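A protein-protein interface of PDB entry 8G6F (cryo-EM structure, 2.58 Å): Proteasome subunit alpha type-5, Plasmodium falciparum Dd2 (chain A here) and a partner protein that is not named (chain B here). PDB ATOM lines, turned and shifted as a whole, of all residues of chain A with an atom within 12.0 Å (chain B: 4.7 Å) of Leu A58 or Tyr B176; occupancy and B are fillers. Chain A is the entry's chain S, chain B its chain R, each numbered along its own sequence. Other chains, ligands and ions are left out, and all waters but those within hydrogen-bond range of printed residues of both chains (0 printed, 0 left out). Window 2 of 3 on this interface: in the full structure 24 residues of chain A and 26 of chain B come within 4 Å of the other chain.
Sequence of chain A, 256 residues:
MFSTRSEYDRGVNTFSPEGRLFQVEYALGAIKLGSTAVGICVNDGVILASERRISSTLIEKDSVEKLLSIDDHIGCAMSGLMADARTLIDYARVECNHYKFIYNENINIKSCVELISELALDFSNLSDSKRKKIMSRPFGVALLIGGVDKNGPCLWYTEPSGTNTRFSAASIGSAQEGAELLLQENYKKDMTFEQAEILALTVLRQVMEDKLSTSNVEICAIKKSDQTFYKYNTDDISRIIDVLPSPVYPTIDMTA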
ATOM      1  N   ARG A  52     -23.321  31.538   9.012  1.00  0.00           N
ATOM      2  CA  ARG A  52     -21.872  31.401   9.015  1.00  0.00           C
ATOM      3  C   ARG A  52     -21.497  30.203   8.158  1.00  0.00           C
ATOM      4  O   ARG A  52     -21.781  29.058   8.527  1.00  0.00           O
ATOM      5  CB  ARG A  52     -21.332  31.235  10.435  1.00  0.00           C
ATOM      6  CG  ARG A  52     -22.071  32.041  11.480  1.00  0.00           C
ATOM      7  CD  ARG A  52     -21.408  31.907  12.837  1.00  0.00           C
ATOM      8  NE  ARG A  52     -20.210  32.731  12.929  1.00  0.00           N
ATOM      9  CZ  ARG A  52     -19.414  32.785  13.986  1.00  0.00           C
ATOM     10  NH1 ARG A  52     -19.655  32.066  15.071  1.00  0.00           N
ATOM     11  NH2 ARG A  52     -18.350  33.581  13.956  1.00  0.00           N
ATOM     12  N   ARG A  53     -20.868  30.469   7.015  1.00  0.00           N
ATOM     13  CA  ARG A  53     -20.379  29.412   6.133  1.00  0.00           C
ATOM     14  C   ARG A  53     -18.960  29.028   6.554  1.00  0.00           C
ATOM     15  O   ARG A  53     -17.974  29.276   5.859  1.00  0.00           O
ATOM     16  CB  ARG A  53     -20.431  29.866   4.682  1.00  0.00           C
ATOM     17  CG  ARG A  53     -21.808  29.798   4.058  1.00  0.00           C
ATOM     18  CD  ARG A  53     -21.806  30.410   2.669  1.00  0.00           C
ATOM     19  NE  ARG A  53     -22.999  30.058   1.911  1.00  0.00           N
ATOM     20  CZ  ARG A  53     -23.391  30.671   0.804  1.00  0.00           C
ATOM     21  NH1 ARG A  53     -22.706  31.681   0.293  1.00  0.00           N
ATOM     22  NH2 ARG A  53     -24.500  30.262   0.194  1.00  0.00           N
ATOM     23  N   ILE A  54     -18.879  28.410   7.731  1.00  0.00           N
ATOM     24  CA  ILE A  54     -17.608  27.967   8.293  1.00  0.00           C
ATOM     25  C   ILE A  54     -16.886  27.109   7.265  1.00  0.00           C
ATOM     26  O   ILE A  54     -17.389  26.059   6.850  1.00  0.00           O
ATOM     27  CB  ILE A  54     -17.823  27.194   9.608  1.00  0.00           C
ATOM     28  CG1 ILE A  54     -18.147  28.156  10.758  1.00  0.00           C
ATOM     29  CG2 ILE A  54     -16.606  26.341   9.935  1.00  0.00           C
ATOM     30  CD1 ILE A  54     -17.055  29.161  11.075  1.00  0.00           C
ATOM     31  N   SER A  55     -15.698  27.552   6.849  1.00  0.00           N
ATOM     32  CA  SER A  55     -14.987  26.865   5.776  1.00  0.00           C
ATOM     33  C   SER A  55     -14.627  25.440   6.175  1.00  0.00           C
ATOM     34  O   SER A  55     -14.936  24.486   5.454  1.00  0.00           O
ATOM     35  CB  SER A  55     -13.732  27.652   5.400  1.00  0.00           C
ATOM     36  OG  SER A  55     -14.065  28.943   4.921  1.00  0.00           O
ATOM     37  N   SER A  56     -13.981  25.276   7.325  1.00  0.00           N
ATOM     38  CA  SER A  56     -13.541  23.964   7.777  1.00  0.00           C
ATOM     39  C   SER A  56     -13.529  23.961   9.300  1.00  0.00           C
ATOM     40  O   SER A  56     -13.981  24.909   9.945  1.00  0.00           O
ATOM     41  CB  SER A  56     -12.168  23.623   7.189  1.00  0.00           C
ATOM     42  OG  SER A  56     -11.136  24.309   7.873  1.00  0.00           O
ATOM     43  N   THR A  57     -13.013  22.878   9.875  1.00  0.00           N
ATOM     44  CA  THR A  57     -12.938  22.742  11.321  1.00  0.00           C
ATOM     45  C   THR A  57     -11.701  23.398  11.917  1.00  0.00           C
ATOM     46  O   THR A  57     -11.647  23.585  13.136  1.00  0.00           O
ATOM     47  CB  THR A  57     -12.969  21.259  11.708  1.00  0.00           C
ATOM     48  OG1 THR A  57     -13.377  21.125  13.074  1.00  0.00           O
ATOM     49  CG2 THR A  57     -11.601  20.625  11.530  1.00  0.00           C
ATOM     50  N   LEU A  58     -10.719  23.759  11.095  1.00  0.00           N
ATOM     51  CA  LEU A  58      -9.491  24.379  11.571  1.00  0.00           C
ATOM     52  C   LEU A  58      -9.575  25.896  11.620  1.00  0.00           C
ATOM     53  O   LEU A  58      -8.609  26.542  12.031  1.00  0.00           O
ATOM     54  CB  LEU A  58      -8.315  23.966  10.683  1.00  0.00           C
ATOM     55  CG  LEU A  58      -7.955  22.480  10.684  1.00  0.00           C
ATOM     56  CD1 LEU A  58      -6.765  22.227   9.782  1.00  0.00           C
ATOM     57  CD2 LEU A  58      -7.669  21.990  12.091  1.00  0.00           C
ATOM     58  N   ILE A  59     -10.696  26.474  11.216  1.00  0.00           N
ATOM     59  CA  ILE A  59     -10.877  27.918  11.258  1.00  0.00           C
ATOM     60  C   ILE A  59     -11.306  28.326  12.659  1.00  0.00           C
ATOM     61  O   ILE A  59     -12.090  27.631  13.314  1.00  0.00           O
ATOM     62  CB  ILE A  59     -11.912  28.354  10.206  1.00  0.00           C
ATOM     63  CG1 ILE A  59     -11.874  29.866  10.002  1.00  0.00           C
ATOM     64  CG2 ILE A  59     -13.302  27.934  10.623  1.00  0.00           C
ATOM     65  CD1 ILE A  59     -10.928  30.307   8.929  1.00  0.00           C
ATOM     66  N   GLU A  60     -10.783  29.455  13.129  1.00  0.00           N
ATOM     67  CA  GLU A  60     -11.225  30.037  14.388  1.00  0.00           C
ATOM     68  C   GLU A  60     -12.492  30.843  14.140  1.00  0.00           C
ATOM     69  O   GLU A  60     -12.480  31.799  13.358  1.00  0.00           O
ATOM     70  CB  GLU A  60     -10.134  30.924  14.978  1.00  0.00           C
ATOM     71  CG  GLU A  60      -8.852  30.197  15.318  1.00  0.00           C
ATOM     72  CD  GLU A  60      -8.897  29.532  16.670  1.00  0.00           C
ATOM     73  OE1 GLU A  60      -9.879  29.747  17.409  1.00  0.00           O
ATOM     74  OE2 GLU A  60      -7.945  28.800  17.004  1.00  0.00           O
ATOM     75  N   LYS A  61     -13.584  30.461  14.805  1.00  0.00           N
ATOM     76  CA  LYS A  61     -14.875  31.074  14.511  1.00  0.00           C
ATOM     77  C   LYS A  61     -14.865  32.567  14.809  1.00  0.00           C
ATOM     78  O   LYS A  61     -15.406  33.368  14.037  1.00  0.00           O
ATOM     79  CB  LYS A  61     -15.974  30.378  15.310  1.00  0.00           C
ATOM     80  CG  LYS A  61     -16.126  28.903  14.993  1.00  0.00           C
ATOM     81  CD  LYS A  61     -17.245  28.277  15.806  1.00  0.00           C
ATOM     82  CE  LYS A  61     -18.607  28.583  15.205  1.00  0.00           C
ATOM     83  NZ  LYS A  61     -19.079  27.492  14.309  1.00  0.00           N
ATOM     84  N   ASP A  62     -14.251  32.963  15.925  1.00  0.00           N
ATOM     85  CA  ASP A  62     -14.273  34.366  16.319  1.00  0.00           C
ATOM     86  C   ASP A  62     -13.611  35.259  15.279  1.00  0.00           C
ATOM     87  O   ASP A  62     -13.950  36.442  15.174  1.00  0.00           O
ATOM     88  CB  ASP A  62     -13.587  34.533  17.672  1.00  0.00           C
ATOM     89  CG  ASP A  62     -14.241  33.704  18.757  1.00  0.00           C
ATOM     90  OD1 ASP A  62     -14.504  32.508  18.513  1.00  0.00           O
ATOM     91  OD2 ASP A  62     -14.495  34.249  19.853  1.00  0.00           O
ATOM     92  N   SER A  63     -12.666  34.721  14.508  1.00  0.00           N
ATOM     93  CA  SER A  63     -11.945  35.541  13.543  1.00  0.00           C
ATOM     94  C   SER A  63     -12.791  35.890  12.329  1.00  0.00           C
ATOM     95  O   SER A  63     -12.413  36.783  11.565  1.00  0.00           O
ATOM     96  CB  SER A  63     -10.677  34.825  13.093  1.00  0.00           C
ATOM     97  OG  SER A  63     -10.989  33.610  12.438  1.00  0.00           O
ATOM     98  N   VAL A  64     -13.912  35.207  12.126  1.00  0.00           N
ATOM     99  CA  VAL A  64     -14.827  35.490  11.028  1.00  0.00           C
ATOM    100  C   VAL A  64     -16.145  35.945  11.632  1.00  0.00           C
ATOM    101  O   VAL A  64     -16.748  35.229  12.442  1.00  0.00           O
ATOM    102  CB  VAL A  64     -15.026  34.270  10.117  1.00  0.00           C
ATOM    103  CG1 VAL A  64     -13.870  34.152   9.138  1.00  0.00           C
ATOM    104  CG2 VAL A  64     -15.173  32.997  10.940  1.00  0.00           C
ATOM    105  N   ILE B  35       1.129  25.296  12.321  1.00  0.00           N
ATOM    106  CA  ILE B  35       0.291  24.609  13.293  1.00  0.00           C
ATOM    107  C   ILE B  35       0.416  25.323  14.629  1.00  0.00           C
ATOM    108  O   ILE B  35       1.502  25.775  15.007  1.00  0.00           O
ATOM    109  CB  ILE B  35       0.671  23.120  13.433  1.00  0.00           C
ATOM    110  CG1 ILE B  35       0.373  22.370  12.135  1.00  0.00           C
ATOM    111  CG2 ILE B  35      -0.103  22.479  14.564  1.00  0.00           C
ATOM    112  CD1 ILE B  35       1.580  22.154  11.266  1.00  0.00           C
ATOM    113  N   LYS B  36      -0.701  25.423  15.340  1.00  0.00           N
ATOM    114  CA  LYS B  36      -0.785  26.132  16.606  1.00  0.00           C
ATOM    115  C   LYS B  36      -0.934  25.139  17.748  1.00  0.00           C
ATOM    116  O   LYS B  36      -1.640  24.134  17.622  1.00  0.00           O
ATOM    117  CB  LYS B  36      -1.970  27.100  16.605  1.00  0.00           C
ATOM    118  CG  LYS B  36      -2.173  27.838  17.907  1.00  0.00           C
ATOM    119  CD  LYS B  36      -3.330  28.810  17.813  1.00  0.00           C
ATOM    120  CE  LYS B  36      -4.663  28.102  17.918  1.00  0.00           C
ATOM    121  NZ  LYS B  36      -5.780  29.057  18.119  1.00  0.00           N
ATOM    122  N   ALA B 155      -8.151  33.772  11.107  1.00  0.00           N
ATOM    123  CA  ALA B 155      -7.357  33.056  12.093  1.00  0.00           C
ATOM    124  C   ALA B 155      -7.634  31.563  12.001  1.00  0.00           C
ATOM    125  O   ALA B 155      -8.751  31.134  11.706  1.00  0.00           O
ATOM    126  CB  ALA B 155      -7.654  33.551  13.506  1.00  0.00           C
ATOM    127  N   TRP B 156      -6.598  30.774  12.260  1.00  0.00           N
ATOM    128  CA  TRP B 156      -6.640  29.334  12.072  1.00  0.00           C
ATOM    129  C   TRP B 156      -6.034  28.632  13.275  1.00  0.00           C
ATOM    130  O   TRP B 156      -5.368  29.240  14.116  1.00  0.00           O
ATOM    131  CB  TRP B 156      -5.887  28.916  10.803  1.00  0.00           C
ATOM    132  CG  TRP B 156      -6.506  29.426   9.557  1.00  0.00           C
ATOM    133  CD1 TRP B 156      -6.316  30.647   8.992  1.00  0.00           C
ATOM    134  CD2 TRP B 156      -7.429  28.733   8.718  1.00  0.00           C
ATOM    135  NE1 TRP B 156      -7.061  30.760   7.850  1.00  0.00           N
ATOM    136  CE2 TRP B 156      -7.756  29.596   7.659  1.00  0.00           C
ATOM    137  CE3 TRP B 156      -8.011  27.464   8.757  1.00  0.00           C
ATOM    138  CZ2 TRP B 156      -8.636  29.234   6.648  1.00  0.00           C
ATOM    139  CZ3 TRP B 156      -8.884  27.108   7.755  1.00  0.00           C
ATOM    140  CH2 TRP B 156      -9.188  27.988   6.714  1.00  0.00           C
ATOM    141  N   LYS B 157      -6.296  27.331  13.353  1.00  0.00           N
ATOM    142  CA  LYS B 157      -5.587  26.440  14.258  1.00  0.00           C
ATOM    143  C   LYS B 157      -4.447  25.711  13.569  1.00  0.00           C
ATOM    144  O   LYS B 157      -3.425  25.436  14.203  1.00  0.00           O
ATOM    145  CB  LYS B 157      -6.555  25.413  14.853  1.00  0.00           C
ATOM    146  CG  LYS B 157      -7.564  26.010  15.810  1.00  0.00           C
ATOM    147  CD  LYS B 157      -8.456  24.944  16.409  1.00  0.00           C
ATOM    148  CE  LYS B 157      -9.659  24.664  15.525  1.00  0.00           C
ATOM    149  NZ  LYS B 157     -10.632  25.785  15.519  1.00  0.00           N
ATOM    150  N   ALA B 158      -4.605  25.402  12.286  1.00  0.00           N
ATOM    151  CA  ALA B 158      -3.538  24.839  11.473  1.00  0.00           C
ATOM    152  C   ALA B 158      -3.890  25.104  10.018  1.00  0.00           C
ATOM    153  O   ALA B 158      -5.021  24.844   9.603  1.00  0.00           O
ATOM    154  CB  ALA B 158      -3.367  23.341  11.729  1.00  0.00           C
ATOM    155  N   GLN B 169      -4.053  20.776   3.679  1.00  0.00           N
ATOM    156  CA  GLN B 169      -5.136  21.187   4.564  1.00  0.00           C
ATOM    157  C   GLN B 169      -6.008  20.002   4.950  1.00  0.00           C
ATOM    158  O   GLN B 169      -6.438  19.888   6.103  1.00  0.00           O
ATOM    159  CB  GLN B 169      -5.977  22.271   3.895  1.00  0.00           C
ATOM    160  CG  GLN B 169      -5.376  23.659   3.980  1.00  0.00           C
ATOM    161  CD  GLN B 169      -6.022  24.630   3.015  1.00  0.00           C
ATOM    162  OE1 GLN B 169      -7.111  24.380   2.503  1.00  0.00           O
ATOM    163  NE2 GLN B 169      -5.349  25.742   2.757  1.00  0.00           N
ATOM    164  N   LEU B 172      -4.166  18.015   7.484  1.00  0.00           N
ATOM    165  CA  LEU B 172      -4.204  18.689   8.776  1.00  0.00           C
ATOM    166  C   LEU B 172      -5.552  18.506   9.457  1.00  0.00           C
ATOM    167  O   LEU B 172      -5.615  18.227  10.658  1.00  0.00           O
ATOM    168  CB  LEU B 172      -3.903  20.174   8.597  1.00  0.00           C
ATOM    169  CG  LEU B 172      -2.463  20.532   8.248  1.00  0.00           C
ATOM    170  CD1 LEU B 172      -2.376  22.000   7.896  1.00  0.00           C
ATOM    171  CD2 LEU B 172      -1.533  20.201   9.396  1.00  0.00           C
ATOM    172  N   GLU B 173      -6.644  18.663   8.709  1.00  0.00           N
ATOM    173  CA  GLU B 173      -7.964  18.456   9.294  1.00  0.00           C
ATOM    174  C   GLU B 173      -8.120  17.033   9.803  1.00  0.00           C
ATOM    175  O   GLU B 173      -8.821  16.799  10.793  1.00  0.00           O
ATOM    176  CB  GLU B 173      -9.051  18.776   8.268  1.00  0.00           C
ATOM    177  CG  GLU B 173      -9.198  20.258   7.979  1.00  0.00           C
ATOM    178  CD  GLU B 173      -9.855  20.532   6.644  1.00  0.00           C
ATOM    179  OE1 GLU B 173     -10.661  19.694   6.191  1.00  0.00           O
ATOM    180  OE2 GLU B 173      -9.558  21.584   6.041  1.00  0.00           O
ATOM    181  N   LYS B 174      -7.477  16.072   9.141  1.00  0.00           N
ATOM    182  CA  LYS B 174      -7.567  14.685   9.581  1.00  0.00           C
ATOM    183  C   LYS B 174      -6.694  14.407  10.801  1.00  0.00           C
ATOM    184  O   LYS B 174      -7.088  13.631  11.678  1.00  0.00           O
ATOM    185  CB  LYS B 174      -7.177  13.751   8.437  1.00  0.00           C
ATOM    186  CG  LYS B 174      -8.191  13.710   7.305  1.00  0.00           C
ATOM    187  CD  LYS B 174      -7.921  12.573   6.328  1.00  0.00           C
ATOM    188  CE  LYS B 174      -8.074  11.206   6.979  1.00  0.00           C
ATOM    189  NZ  LYS B 174      -9.365  11.065   7.709  1.00  0.00           N
ATOM    190  N   ASN B 175      -5.511  15.024  10.880  1.00  0.00           N
ATOM    191  CA  ASN B 175      -4.493  14.626  11.847  1.00  0.00           C
ATOM    192  C   ASN B 175      -4.184  15.703  12.882  1.00  0.00           C
ATOM    193  O   ASN B 175      -3.151  15.621  13.551  1.00  0.00           O
ATOM    194  CB  ASN B 175      -3.201  14.240  11.125  1.00  0.00           C
ATOM    195  CG  ASN B 175      -3.413  13.172  10.080  1.00  0.00           C
ATOM    196  OD1 ASN B 175      -3.258  11.983  10.352  1.00  0.00           O
ATOM    197  ND2 ASN B 175      -3.767  13.588   8.874  1.00  0.00           N
ATOM    198  N   TYR B 176      -5.041  16.707  13.039  1.00  0.00           N
ATOM    199  CA  TYR B 176      -4.777  17.779  13.988  1.00  0.00           C
ATOM    200  C   TYR B 176      -5.413  17.479  15.338  1.00  0.00           C
ATOM    201  O   TYR B 176      -6.554  17.019  15.415  1.00  0.00           O
ATOM    202  CB  TYR B 176      -5.302  19.116  13.467  1.00  0.00           C
ATOM    203  CG  TYR B 176      -5.134  20.247  14.456  1.00  0.00           C
ATOM    204  CD1 TYR B 176      -3.879  20.748  14.759  1.00  0.00           C
ATOM    205  CD2 TYR B 176      -6.230  20.809  15.091  1.00  0.00           C
ATOM    206  CE1 TYR B 176      -3.718  21.775  15.662  1.00  0.00           C
ATOM    207  CE2 TYR B 176      -6.079  21.838  15.997  1.00  0.00           C
ATOM    208  CZ  TYR B 176      -4.821  22.317  16.277  1.00  0.00           C
ATOM    209  OH  TYR B 176      -4.663  23.343  17.177  1.00  0.00           O
ATOM    210  N   GLN B 177      -4.661  17.749  16.400  1.00  0.00           N
ATOM    211  CA  GLN B 177      -5.144  17.618  17.765  1.00  0.00           C
ATOM    212  C   GLN B 177      -4.811  18.886  18.532  1.00  0.00           C
ATOM    213  O   GLN B 177      -3.820  19.560  18.249  1.00  0.00           O
ATOM    214  CB  GLN B 177      -4.521  16.415  18.476  1.00  0.00           C
ATOM    215  CG  GLN B 177      -5.028  15.070  17.991  1.00  0.00           C
ATOM    216  CD  GLN B 177      -4.051  13.952  18.282  1.00  0.00           C
ATOM    217  OE1 GLN B 177      -2.999  14.172  18.885  1.00  0.00           O
ATOM    218  NE2 GLN B 177      -4.393  12.742  17.858  1.00  0.00           N
ATOM    219  N   GLU B 178      -5.647  19.201  19.513  1.00  0.00           N
ATOM    220  CA  GLU B 178      -5.457  20.401  20.310  1.00  0.00           C
ATOM    221  C   GLU B 178      -4.450  20.151  21.422  1.00  0.00           C
ATOM    222  O   GLU B 178      -4.428  19.078  22.032  1.00  0.00           O
ATOM    223  CB  GLU B 178      -6.789  20.856  20.902  1.00  0.00           C
ATOM    224  CG  GLU B 178      -6.892  22.360  21.128  1.00  0.00           C
ATOM    225  CD  GLU B 178      -8.237  22.933  20.713  1.00  0.00           C
ATOM    226  OE1 GLU B 178      -9.030  22.216  20.070  1.00  0.00           O
ATOM    227  OE2 GLU B 178      -8.500  24.111  21.029  1.00  0.00           O
ATOM    228  N   LEU B 188       3.930  16.452  13.206  1.00  0.00           N
ATOM    229  CA  LEU B 188       2.731  16.689  12.411  1.00  0.00           C
ATOM    230  C   LEU B 188       3.009  17.668  11.280  1.00  0.00           C
ATOM    231  O   LEU B 188       2.564  17.461  10.145  1.00  0.00           O
ATOM    232  CB  LEU B 188       1.609  17.208  13.307  1.00  0.00           C
ATOM    233  CG  LEU B 188       0.284  17.533  12.620  1.00  0.00           C
ATOM    234  CD1 LEU B 188      -0.281  16.304  11.937  1.00  0.00           C
ATOM    235  CD2 LEU B 188      -0.705  18.087  13.623  1.00  0.00           C
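Of the 13 printed residues of chain A, 6 touch a printed residue of chain B.
Hydrophobic or aromatic side chains of chain A that line the printed part of chain B: Leu A58 and Ile A59.
Of the 15 printed residues of chain B, 8 touch a printed residue of chain A.
Printed residues of chain B that touch a printed residue of chain A: Lys B36, Ala B155, Trp B156, Lys B157, Ala B158, Leu B172, Glu B173 and Tyr B176.
Hydrophobic or aromatic side chains of chain B that line the printed part of chain A: Ala B155, Trp B156, Leu B172 and Tyr B176.
Among the printed residues, 17 pairs touch across the chains.
Among the printed residues, Asp or Glu carboxylates within 4 Å of a Lys or Arg side-chain nitrogen of the other chain: Glu A60 with Lys B36.
The side-chain amino group (NZ) of Lys B36 lies within salt-bridge range of the side-chain carboxylate (OE2) of Glu A60, at 2.4 Å.
N of Glu A60 lies within hydrogen-bond range of O of Ala B155, at 3.0 Å.
N of Ala B155 is in hydrogen-bond range of OG of Ser A63, 3.1 Å away.
The side-chain amino group (NZ) of Lys B157 sits close to the backbone carbonyl oxygen (O) of Thr A57, 3.4 Å away.
The backbone NH (N) of Lys B157 is in hydrogen-bond range of the backbone carbonyl oxygen (O) of Leu A58 (2.8 Å).
NZ of Lys B157 is in hydrogen-bond range of O of Ile A59 (3.2 Å).
OG of Ser A56 touches CZ3 of Trp B156, 3.6 Å away.
Trp B156 touches Leu A58.
O of Ala B158 touches CD1 of Leu A58, at 3.1 Å.
CB of Leu B172 touches CD1 of Leu A58 (3.7 Å).
Glu B173 touches Leu A58 (CG to CD1, 3.6 Å).
CD2 of Tyr B176 touches CD2 of Leu A58, at 3.5 Å.
Ile A59 touches Ala B155.
CZ2 of Trp B156 touches CD1 of Ile A59, 3.4 Å away.
Glu A60 touches Trp B156.
CG of Lys B157 touches OE2 of Glu A60, at 3.1 Å.
Arg A53 touches none of the printed residues of chain B.
Ile A54 touches none of the printed residues of chain B.
Of the printed residues of chain B, Ser A56 touches Trp B156 (3.6 Å) and Glu B173 (3.5 Å).
Printed residues of chain B within 4 Å of Thr A57: Lys B157.
Of chain B, only Trp B156, Lys B157, Ala B158, Leu B172, Glu B173 and Tyr B176 come within 4 Å of Leu A58.
Of the printed residues of chain B, Ile A59 touches Ala B155 (3.6 Å), Trp B156 (3.4 Å) and Lys B157 (3.2 Å).
Of the printed residues of chain B, Glu A60 touches Lys B36, Ala B155, Trp B156 and Lys B157.
Lys B36 touches just one residue of chain A: Glu A60 (2.4 Å).
Ala B155 touches three residues of chain A.
Trp B156 touches just these residues of chain A: Ser A56 (3.6 Å), Leu A58 (3.4 Å), Ile A59 (3.4 Å) and Glu A60 (3.8 Å).
Ala B158 touches one residue of chain A.
Of chain A, only Leu A58 (3.7 Å) comes within 4 Å of Leu B172.
No residue of chain A comes within 4 Å of Asn B175.
Of the printed residues of chain A, Tyr B176 touches Leu A58.
No residue of chain A comes within 4 Å of Gln B177.
Glu B178 touches none of the printed residues of chain A.
The nearest printed residue of chain B that does not touch Glu A60 is Glu B178 (6.2 Å).
The backbone NH (N) of Lys B36 is in hydrogen-bond range of the backbone carbonyl oxygen (O) of Lys B157.
OH of Tyr B176 lies within hydrogen-bond range of O of Lys B36.
The side-chain hydroxyl (OG) of Ser A56 sits at hydrogen-bond distance from the backbone NH (N) of Leu A58, at 3.3 Å.
The side-chain hydroxyl of Ser A63 is in hydrogen-bond range of the backbone carbonyl oxygen of Glu A60.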
